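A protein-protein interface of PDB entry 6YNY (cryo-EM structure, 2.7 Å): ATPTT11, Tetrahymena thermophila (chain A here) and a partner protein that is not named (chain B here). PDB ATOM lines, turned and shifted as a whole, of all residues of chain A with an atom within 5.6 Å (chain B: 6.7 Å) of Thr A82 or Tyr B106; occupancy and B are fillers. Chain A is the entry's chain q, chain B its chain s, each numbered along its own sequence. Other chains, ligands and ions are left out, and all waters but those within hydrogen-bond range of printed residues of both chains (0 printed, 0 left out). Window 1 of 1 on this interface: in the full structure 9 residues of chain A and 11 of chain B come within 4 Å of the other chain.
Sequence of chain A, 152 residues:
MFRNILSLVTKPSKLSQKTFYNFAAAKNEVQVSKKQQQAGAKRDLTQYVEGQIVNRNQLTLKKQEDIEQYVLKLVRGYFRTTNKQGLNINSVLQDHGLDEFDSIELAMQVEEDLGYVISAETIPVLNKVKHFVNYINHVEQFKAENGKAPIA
The backbone NH (N) of Lys A84 sits close to the backbone carbonyl oxygen (O) of Glu B98, at 3.2 Å. OG1 of Thr A82 lies close to O of Ser B103 (2.4 Å). The side-chain hydroxyl (OH) of Tyr B106 is in hydrogen-bond range of the side-chain amino group (NZ) of Lys A84 (3.0 Å). The guanidinium group (NH2) of Arg A80 lies within salt-bridge range of the side-chain carboxylate (OD2) of Asp B74 (2.9 Å). The side-chain hydroxyl (OH) of Tyr B106 lies close to the backbone carbonyl oxygen (O) of Thr A81 (2.3 Å). The backbone carbonyl oxygen (O) of Asn B104 lies close to the backbone NH (N) of Gly A97, at 3.2 Å.
NZ of Lys B81 is in salt-bridge range of OE1 of Glu B98 (3.7 Å). The side-chain hydroxyl of Thr B105 lies close to the backbone NH of Ile B107 (3.3 Å). The side-chain amino group (NZ) of Lys A84 is in hydrogen-bond range of the backbone carbonyl oxygen (O) of Thr A81, 2.8 Å away. OG of Ser B103 sits at hydrogen-bond distance from O of Thr B105 (3.0 Å). The side-chain carboxylate of Asp B74 is in hydrogen-bond range of the indole nitrogen of Trp B77 (3.2 Å). The backbone carbonyl oxygen of Thr A82 sits at hydrogen-bond distance from a ring nitrogen (ND1) of His A96 (2.7 Å).
Tyr B78 touches Phe A79. Phe A79 touches Tyr B106. Arg A80 touches Tyr B106. Thr A82 touches Asn B104. Thr B105 touches Thr A82. OH of Tyr B106 touches CA of Thr A82, at 3.7 Å. Asn B99 touches Asn A83. Asn A83 touches Ile B101 (CB to O, 3.4 Å). CD of Lys A84 touches OD1 of Asn B99 (3.3 Å). O of Asp A95 touches CA of Asn B104 (3.6 Å).
Of the printed residues of chain A, Asp B74 touches Arg A80. Printed residues of chain A within 4 Å of Tyr B78: Phe A79 (3.9 Å). Of the printed residues of chain A, Asn B99 touches Asn A83 (3.5 Å) and Lys A84 (3.3 Å). Of chain A, only Phe A79 (3.7 Å), Arg A80 (3.9 Å), Thr A81 (2.3 Å), Thr A82 (3.7 Å) and Lys A84 (3.0 Å) come within 4 Å of Tyr B106. Leu B108 touches none of the printed residues of chain A. The nearest residue of chain B that does not touch Thr A82 is Glu B98 (4.5 Å).
Hydrophobic or aromatic side chains of chain A within 4 Å of the printed part of chain B: Phe A79. Along chain A the printed residues that touch a printed residue of chain B span positions 79 to 97. Of the 17 printed residues of chain B, 11 touch a printed residue of chain A. Hydrophobic or aromatic side chains of chain B that line the printed part of chain A: Trp B77, Tyr B78, Ala B102 and Tyr B106. Among the printed residues, 19 pairs touch across the chains. Among the printed residues, Asp or Glu carboxylates within 4 Å of a Lys or Arg side-chain nitrogen of the other chain: Arg A80 with Asp B74.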
ATOM      1  N   PHE A  79       2.365 -23.067 -20.823  1.00  0.00           N
ATOM      2  CA  PHE A  79       1.337 -22.644 -19.882  1.00  0.00           C
ATOM      3  C   PHE A  79       0.356 -21.643 -20.475  1.00  0.00           C
ATOM      4  O   PHE A  79      -0.674 -21.373 -19.849  1.00  0.00           O
ATOM      5  CB  PHE A  79       1.997 -22.046 -18.640  1.00  0.00           C
ATOM      6  CG  PHE A  79       2.587 -20.684 -18.857  1.00  0.00           C
ATOM      7  CD1 PHE A  79       1.992 -19.566 -18.311  1.00  0.00           C
ATOM      8  CD2 PHE A  79       3.734 -20.522 -19.606  1.00  0.00           C
ATOM      9  CE1 PHE A  79       2.529 -18.317 -18.505  1.00  0.00           C
ATOM     10  CE2 PHE A  79       4.274 -19.273 -19.803  1.00  0.00           C
ATOM     11  CZ  PHE A  79       3.671 -18.172 -19.253  1.00  0.00           C
ATOM     12  N   ARG A  80       0.641 -21.095 -21.650  1.00  0.00           N
ATOM     13  CA  ARG A  80      -0.244 -20.136 -22.293  1.00  0.00           C
ATOM     14  C   ARG A  80      -1.231 -20.781 -23.252  1.00  0.00           C
ATOM     15  O   ARG A  80      -2.135 -20.093 -23.739  1.00  0.00           O
ATOM     16  CB  ARG A  80       0.577 -19.102 -23.061  1.00  0.00           C
ATOM     17  CG  ARG A  80       1.513 -18.271 -22.212  1.00  0.00           C
ATOM     18  CD  ARG A  80       0.953 -16.896 -21.967  1.00  0.00           C
ATOM     19  NE  ARG A  80       0.663 -16.203 -23.215  1.00  0.00           N
ATOM     20  CZ  ARG A  80      -0.040 -15.082 -23.295  1.00  0.00           C
ATOM     21  NH1 ARG A  80      -0.261 -14.527 -24.475  1.00  0.00           N
ATOM     22  NH2 ARG A  80      -0.522 -14.518 -22.199  1.00  0.00           N
ATOM     23  N   THR A  81      -1.086 -22.070 -23.536  1.00  0.00           N
ATOM     24  CA  THR A  81      -1.893 -22.723 -24.553  1.00  0.00           C
ATOM     25  C   THR A  81      -3.290 -23.023 -24.027  1.00  0.00           C
ATOM     26  O   THR A  81      -3.449 -23.547 -22.921  1.00  0.00           O
ATOM     27  CB  THR A  81      -1.216 -24.012 -25.008  1.00  0.00           C
ATOM     28  OG1 THR A  81       0.125 -23.730 -25.417  1.00  0.00           O
ATOM     29  CG2 THR A  81      -1.964 -24.628 -26.161  1.00  0.00           C
ATOM     30  N   THR A  82      -4.298 -22.694 -24.829  1.00  0.00           N
ATOM     31  CA  THR A  82      -5.687 -22.993 -24.529  1.00  0.00           C
ATOM     32  C   THR A  82      -6.184 -24.118 -25.427  1.00  0.00           C
ATOM     33  O   THR A  82      -5.675 -24.324 -26.532  1.00  0.00           O
ATOM     34  CB  THR A  82      -6.578 -21.764 -24.725  1.00  0.00           C
ATOM     35  OG1 THR A  82      -6.676 -21.458 -26.119  1.00  0.00           O
ATOM     36  CG2 THR A  82      -6.010 -20.573 -23.997  1.00  0.00           C
ATOM     37  N   ASN A  83      -7.188 -24.840 -24.941  1.00  0.00           N
ATOM     38  CA  ASN A  83      -7.799 -25.941 -25.675  1.00  0.00           C
ATOM     39  C   ASN A  83      -6.735 -26.935 -26.137  1.00  0.00           C
ATOM     40  O   ASN A  83      -6.541 -27.183 -27.327  1.00  0.00           O
ATOM     41  CB  ASN A  83      -8.612 -25.408 -26.855  1.00  0.00           C
ATOM     42  CG  ASN A  83      -9.466 -26.468 -27.499  1.00  0.00           C
ATOM     43  OD1 ASN A  83      -9.558 -27.593 -27.011  1.00  0.00           O
ATOM     44  ND2 ASN A  83     -10.111 -26.111 -28.599  1.00  0.00           N
ATOM     45  N   LYS A  84      -6.045 -27.514 -25.154  1.00  0.00           N
ATOM     46  CA  LYS A  84      -4.923 -28.391 -25.458  1.00  0.00           C
ATOM     47  C   LYS A  84      -5.365 -29.649 -26.191  1.00  0.00           C
ATOM     48  O   LYS A  84      -4.608 -30.185 -27.008  1.00  0.00           O
ATOM     49  CB  LYS A  84      -4.193 -28.761 -24.170  1.00  0.00           C
ATOM     50  CG  LYS A  84      -3.493 -27.597 -23.506  1.00  0.00           C
ATOM     51  CD  LYS A  84      -2.842 -28.009 -22.204  1.00  0.00           C
ATOM     52  CE  LYS A  84      -1.931 -26.928 -21.656  1.00  0.00           C
ATOM     53  NZ  LYS A  84      -2.643 -25.664 -21.358  1.00  0.00           N
ATOM     54  N   ASP A  95      -5.253 -19.292 -32.475  1.00  0.00           N
ATOM     55  CA  ASP A  95      -6.532 -19.765 -31.970  1.00  0.00           C
ATOM     56  C   ASP A  95      -6.411 -20.465 -30.626  1.00  0.00           C
ATOM     57  O   ASP A  95      -7.419 -20.961 -30.112  1.00  0.00           O
ATOM     58  CB  ASP A  95      -7.171 -20.713 -32.985  1.00  0.00           C
ATOM     59  CG  ASP A  95      -7.455 -20.042 -34.310  1.00  0.00           C
ATOM     60  OD1 ASP A  95      -7.229 -18.819 -34.419  1.00  0.00           O
ATOM     61  OD2 ASP A  95      -7.900 -20.738 -35.246  1.00  0.00           O
ATOM     62  N   HIS A  96      -5.210 -20.519 -30.050  1.00  0.00           N
ATOM     63  CA  HIS A  96      -4.986 -21.178 -28.771  1.00  0.00           C
ATOM     64  C   HIS A  96      -4.278 -20.263 -27.777  1.00  0.00           C
ATOM     65  O   HIS A  96      -3.626 -20.752 -26.850  1.00  0.00           O
ATOM     66  CB  HIS A  96      -4.193 -22.469 -28.970  1.00  0.00           C
ATOM     67  CG  HIS A  96      -4.906 -23.487 -29.802  1.00  0.00           C
ATOM     68  ND1 HIS A  96      -5.555 -24.571 -29.255  1.00  0.00           N
ATOM     69  CD2 HIS A  96      -5.081 -23.582 -31.141  1.00  0.00           C
ATOM     70  CE1 HIS A  96      -6.095 -25.293 -30.220  1.00  0.00           C
ATOM     71  NE2 HIS A  96      -5.822 -24.714 -31.375  1.00  0.00           N
ATOM     72  N   GLY A  97      -4.384 -18.951 -27.957  1.00  0.00           N
ATOM     73  CA  GLY A  97      -3.831 -18.014 -27.001  1.00  0.00           C
ATOM     74  C   GLY A  97      -2.348 -17.776 -27.124  1.00  0.00           C
ATOM     75  O   GLY A  97      -1.696 -17.459 -26.126  1.00  0.00           O
ATOM     76  N   ASP B  74      -3.376 -11.157 -17.829  1.00  0.00           N
ATOM     77  CA  ASP B  74      -2.998 -12.562 -17.760  1.00  0.00           C
ATOM     78  C   ASP B  74      -2.660 -12.995 -16.341  1.00  0.00           C
ATOM     79  O   ASP B  74      -2.817 -14.171 -16.002  1.00  0.00           O
ATOM     80  CB  ASP B  74      -1.813 -12.829 -18.686  1.00  0.00           C
ATOM     81  CG  ASP B  74      -2.148 -12.614 -20.143  1.00  0.00           C
ATOM     82  OD1 ASP B  74      -3.251 -13.010 -20.568  1.00  0.00           O
ATOM     83  OD2 ASP B  74      -1.303 -12.049 -20.867  1.00  0.00           O
ATOM     84  N   TRP B  77      -5.622 -15.028 -14.378  1.00  0.00           N
ATOM     85  CA  TRP B  77      -5.869 -16.449 -14.563  1.00  0.00           C
ATOM     86  C   TRP B  77      -4.669 -17.295 -14.178  1.00  0.00           C
ATOM     87  O   TRP B  77      -4.841 -18.468 -13.840  1.00  0.00           O
ATOM     88  CB  TRP B  77      -6.282 -16.747 -16.006  1.00  0.00           C
ATOM     89  CG  TRP B  77      -5.272 -16.439 -17.073  1.00  0.00           C
ATOM     90  CD1 TRP B  77      -5.274 -15.365 -17.906  1.00  0.00           C
ATOM     91  CD2 TRP B  77      -4.134 -17.228 -17.442  1.00  0.00           C
ATOM     92  NE1 TRP B  77      -4.211 -15.427 -18.764  1.00  0.00           N
ATOM     93  CE2 TRP B  77      -3.492 -16.560 -18.499  1.00  0.00           C
ATOM     94  CE3 TRP B  77      -3.594 -18.428 -16.981  1.00  0.00           C
ATOM     95  CZ2 TRP B  77      -2.338 -17.049 -19.098  1.00  0.00           C
ATOM     96  CZ3 TRP B  77      -2.447 -18.909 -17.574  1.00  0.00           C
ATOM     97  CH2 TRP B  77      -1.832 -18.223 -18.622  1.00  0.00           C
ATOM     98  N   TYR B  78      -3.464 -16.729 -14.212  1.00  0.00           N
ATOM     99  CA  TYR B  78      -2.292 -17.484 -13.791  1.00  0.00           C
ATOM    100  C   TYR B  78      -2.268 -17.645 -12.281  1.00  0.00           C
ATOM    101  O   TYR B  78      -1.925 -18.717 -11.767  1.00  0.00           O
ATOM    102  CB  TYR B  78      -1.022 -16.793 -14.277  1.00  0.00           C
ATOM    103  CG  TYR B  78       0.237 -17.544 -13.938  1.00  0.00           C
ATOM    104  CD1 TYR B  78       0.667 -18.599 -14.723  1.00  0.00           C
ATOM    105  CD2 TYR B  78       0.995 -17.202 -12.834  1.00  0.00           C
ATOM    106  CE1 TYR B  78       1.810 -19.288 -14.416  1.00  0.00           C
ATOM    107  CE2 TYR B  78       2.140 -17.887 -12.522  1.00  0.00           C
ATOM    108  CZ  TYR B  78       2.545 -18.928 -13.317  1.00  0.00           C
ATOM    109  OH  TYR B  78       3.686 -19.622 -13.015  1.00  0.00           O
ATOM    110  N   LYS B  81      -5.154 -20.187 -11.132  1.00  0.00           N
ATOM    111  CA  LYS B  81      -4.764 -21.590 -11.189  1.00  0.00           C
ATOM    112  C   LYS B  81      -3.894 -21.968  -9.999  1.00  0.00           C
ATOM    113  O   LYS B  81      -4.045 -23.054  -9.430  1.00  0.00           O
ATOM    114  CB  LYS B  81      -4.025 -21.874 -12.491  1.00  0.00           C
ATOM    115  CG  LYS B  81      -4.870 -21.738 -13.724  1.00  0.00           C
ATOM    116  CD  LYS B  81      -4.071 -22.086 -14.955  1.00  0.00           C
ATOM    117  CE  LYS B  81      -4.894 -21.959 -16.207  1.00  0.00           C
ATOM    118  NZ  LYS B  81      -4.124 -22.362 -17.403  1.00  0.00           N
ATOM    119  N   VAL B  94      -9.171 -26.596 -13.322  1.00  0.00           N
ATOM    120  CA  VAL B  94      -8.033 -26.192 -14.140  1.00  0.00           C
ATOM    121  C   VAL B  94      -7.815 -27.183 -15.273  1.00  0.00           C
ATOM    122  O   VAL B  94      -7.762 -26.807 -16.450  1.00  0.00           O
ATOM    123  CB  VAL B  94      -6.776 -26.049 -13.264  1.00  0.00           C
ATOM    124  CG1 VAL B  94      -5.569 -25.762 -14.116  1.00  0.00           C
ATOM    125  CG2 VAL B  94      -6.971 -24.952 -12.245  1.00  0.00           C
ATOM    126  N   VAL B  97     -10.567 -26.978 -17.852  1.00  0.00           N
ATOM    127  CA  VAL B  97     -10.644 -25.717 -18.579  1.00  0.00           C
ATOM    128  C   VAL B  97      -9.530 -25.620 -19.610  1.00  0.00           C
ATOM    129  O   VAL B  97      -9.750 -25.176 -20.742  1.00  0.00           O
ATOM    130  CB  VAL B  97     -10.603 -24.541 -17.590  1.00  0.00           C
ATOM    131  CG1 VAL B  97     -10.326 -23.243 -18.318  1.00  0.00           C
ATOM    132  CG2 VAL B  97     -11.904 -24.457 -16.833  1.00  0.00           C
ATOM    133  N   GLU B  98      -8.322 -26.028 -19.242  1.00  0.00           N
ATOM    134  CA  GLU B  98      -7.182 -25.916 -20.138  1.00  0.00           C
ATOM    135  C   GLU B  98      -7.148 -27.009 -21.192  1.00  0.00           C
ATOM    136  O   GLU B  98      -6.231 -27.017 -22.019  1.00  0.00           O
ATOM    137  CB  GLU B  98      -5.883 -25.936 -19.329  1.00  0.00           C
ATOM    138  CG  GLU B  98      -5.578 -27.262 -18.676  1.00  0.00           C
ATOM    139  CD  GLU B  98      -4.421 -27.171 -17.702  1.00  0.00           C
ATOM    140  OE1 GLU B  98      -4.002 -26.039 -17.380  1.00  0.00           O
ATOM    141  OE2 GLU B  98      -3.927 -28.230 -17.259  1.00  0.00           O
ATOM    142  N   ASN B  99      -8.107 -27.919 -21.187  1.00  0.00           N
ATOM    143  CA  ASN B  99      -8.123 -29.027 -22.131  1.00  0.00           C
ATOM    144  C   ASN B  99      -9.440 -29.175 -22.877  1.00  0.00           C
ATOM    145  O   ASN B  99      -9.430 -29.548 -24.051  1.00  0.00           O
ATOM    146  CB  ASN B  99      -7.804 -30.329 -21.392  1.00  0.00           C
ATOM    147  CG  ASN B  99      -6.416 -30.331 -20.796  1.00  0.00           C
ATOM    148  OD1 ASN B  99      -5.520 -29.646 -21.282  1.00  0.00           O
ATOM    149  ND2 ASN B  99      -6.229 -31.104 -19.740  1.00  0.00           N
ATOM    150  N   ILE B 101     -12.119 -26.791 -23.266  1.00  0.00           N
ATOM    151  CA  ILE B 101     -12.843 -25.547 -23.501  1.00  0.00           C
ATOM    152  C   ILE B 101     -12.231 -24.865 -24.714  1.00  0.00           C
ATOM    153  O   ILE B 101     -11.040 -24.538 -24.711  1.00  0.00           O
ATOM    154  CB  ILE B 101     -12.818 -24.613 -22.281  1.00  0.00           C
ATOM    155  CG1 ILE B 101     -13.679 -25.214 -21.172  1.00  0.00           C
ATOM    156  CG2 ILE B 101     -13.312 -23.227 -22.660  1.00  0.00           C
ATOM    157  CD1 ILE B 101     -13.748 -24.391 -19.932  1.00  0.00           C
ATOM    158  N   ALA B 102     -13.043 -24.648 -25.745  1.00  0.00           N
ATOM    159  CA  ALA B 102     -12.589 -24.041 -26.992  1.00  0.00           C
ATOM    160  C   ALA B 102     -12.599 -22.531 -26.831  1.00  0.00           C
ATOM    161  O   ALA B 102     -13.564 -21.849 -27.176  1.00  0.00           O
ATOM    162  CB  ALA B 102     -13.471 -24.481 -28.151  1.00  0.00           C
ATOM    163  N   SER B 103     -11.504 -21.999 -26.296  1.00  0.00           N
ATOM    164  CA  SER B 103     -11.343 -20.567 -26.118  1.00  0.00           C
ATOM    165  C   SER B 103      -9.951 -20.165 -26.571  1.00  0.00           C
ATOM    166  O   SER B 103      -8.978 -20.885 -26.330  1.00  0.00           O
ATOM    167  CB  SER B 103     -11.565 -20.156 -24.662  1.00  0.00           C
ATOM    168  OG  SER B 103     -11.644 -18.748 -24.536  1.00  0.00           O
ATOM    169  N   ASN B 104      -9.864 -19.017 -27.229  1.00  0.00           N
ATOM    170  CA  ASN B 104      -8.601 -18.499 -27.728  1.00  0.00           C
ATOM    171  C   ASN B 104      -7.817 -17.740 -26.671  1.00  0.00           C
ATOM    172  O   ASN B 104      -6.793 -17.134 -26.998  1.00  0.00           O
ATOM    173  CB  ASN B 104      -8.846 -17.589 -28.931  1.00  0.00           C
ATOM    174  CG  ASN B 104      -9.758 -16.431 -28.602  1.00  0.00           C
ATOM    175  OD1 ASN B 104     -10.694 -16.567 -27.816  1.00  0.00           O
ATOM    176  ND2 ASN B 104      -9.490 -15.280 -29.198  1.00  0.00           N
ATOM    177  N   THR B 105      -8.272 -17.754 -25.423  1.00  0.00           N
ATOM    178  CA  THR B 105      -7.595 -17.034 -24.358  1.00  0.00           C
ATOM    179  C   THR B 105      -8.143 -17.504 -23.022  1.00  0.00           C
ATOM    180  O   THR B 105      -9.304 -17.909 -22.922  1.00  0.00           O
ATOM    181  CB  THR B 105      -7.783 -15.520 -24.499  1.00  0.00           C
ATOM    182  OG1 THR B 105      -7.063 -14.845 -23.461  1.00  0.00           O
ATOM    183  CG2 THR B 105      -9.250 -15.155 -24.408  1.00  0.00           C
ATOM    184  N   TYR B 106      -7.294 -17.442 -22.000  1.00  0.00           N
ATOM    185  CA  TYR B 106      -7.700 -17.770 -20.643  1.00  0.00           C
ATOM    186  C   TYR B 106      -8.358 -16.602 -19.927  1.00  0.00           C
ATOM    187  O   TYR B 106      -8.835 -16.779 -18.802  1.00  0.00           O
ATOM    188  CB  TYR B 106      -6.495 -18.245 -19.834  1.00  0.00           C
ATOM    189  CG  TYR B 106      -6.033 -19.645 -20.144  1.00  0.00           C
ATOM    190  CD1 TYR B 106      -6.920 -20.706 -20.144  1.00  0.00           C
ATOM    191  CD2 TYR B 106      -4.706 -19.907 -20.434  1.00  0.00           C
ATOM    192  CE1 TYR B 106      -6.500 -21.984 -20.422  1.00  0.00           C
ATOM    193  CE2 TYR B 106      -4.277 -21.179 -20.714  1.00  0.00           C
ATOM    194  CZ  TYR B 106      -5.177 -22.215 -20.709  1.00  0.00           C
ATOM    195  OH  TYR B 106      -4.747 -23.488 -20.990  1.00  0.00           O
ATOM    196  N   ILE B 107      -8.395 -15.421 -20.539  1.00  0.00           N
ATOM    197  CA  ILE B 107      -9.080 -14.269 -19.959  1.00  0.00           C
ATOM    198  C   ILE B 107     -10.540 -14.403 -20.375  1.00  0.00           C
ATOM    199  O   ILE B 107     -10.977 -13.869 -21.394  1.00  0.00           O
ATOM    200  CB  ILE B 107      -8.467 -12.947 -20.408  1.00  0.00           C
ATOM    201  CG1 ILE B 107      -6.970 -12.931 -20.115  1.00  0.00           C
ATOM    202  CG2 ILE B 107      -9.139 -11.791 -19.702  1.00  0.00           C
ATOM    203  CD1 ILE B 107      -6.281 -11.680 -20.568  1.00  0.00           C
ATOM    204  N   LEU B 108     -11.299 -15.130 -19.566  1.00  0.00           N
ATOM    205  CA  LEU B 108     -12.695 -15.400 -19.865  1.00  0.00           C
ATOM    206  C   LEU B 108     -13.554 -14.201 -19.495  1.00  0.00           C
ATOM    207  O   LEU B 108     -13.508 -13.717 -18.362  1.00  0.00           O
ATOM    208  CB  LEU B 108     -13.161 -16.643 -19.115  1.00  0.00           C
ATOM    209  CG  LEU B 108     -12.348 -17.904 -19.410  1.00  0.00           C
ATOM    210  CD1 LEU B 108     -12.870 -19.074 -18.617  1.00  0.00           C
ATOM    211  CD2 LEU B 108     -12.374 -18.212 -20.885  1.00  0.00           C
ATOM    212  N   ILE B 109     -14.334 -13.724 -20.459  1.00  0.00           N
ATOM    213  CA  ILE B 109     -15.237 -12.600 -20.266  1.00  0.00           C
ATOM    214  C   ILE B 109     -16.604 -13.016 -20.780  1.00  0.00           C
ATOM    215  O   ILE B 109     -16.748 -13.372 -21.955  1.00  0.00           O
ATOM    216  CB  ILE B 109     -14.746 -11.335 -20.985  1.00  0.00           C
ATOM    217  CG1 ILE B 109     -13.375 -10.934 -20.446  1.00  0.00           C
ATOM    218  CG2 ILE B 109     -15.735 -10.206 -20.798  1.00  0.00           C
ATOM    219  CD1 ILE B 109     -12.739  -9.782 -21.166  1.00  0.00           C
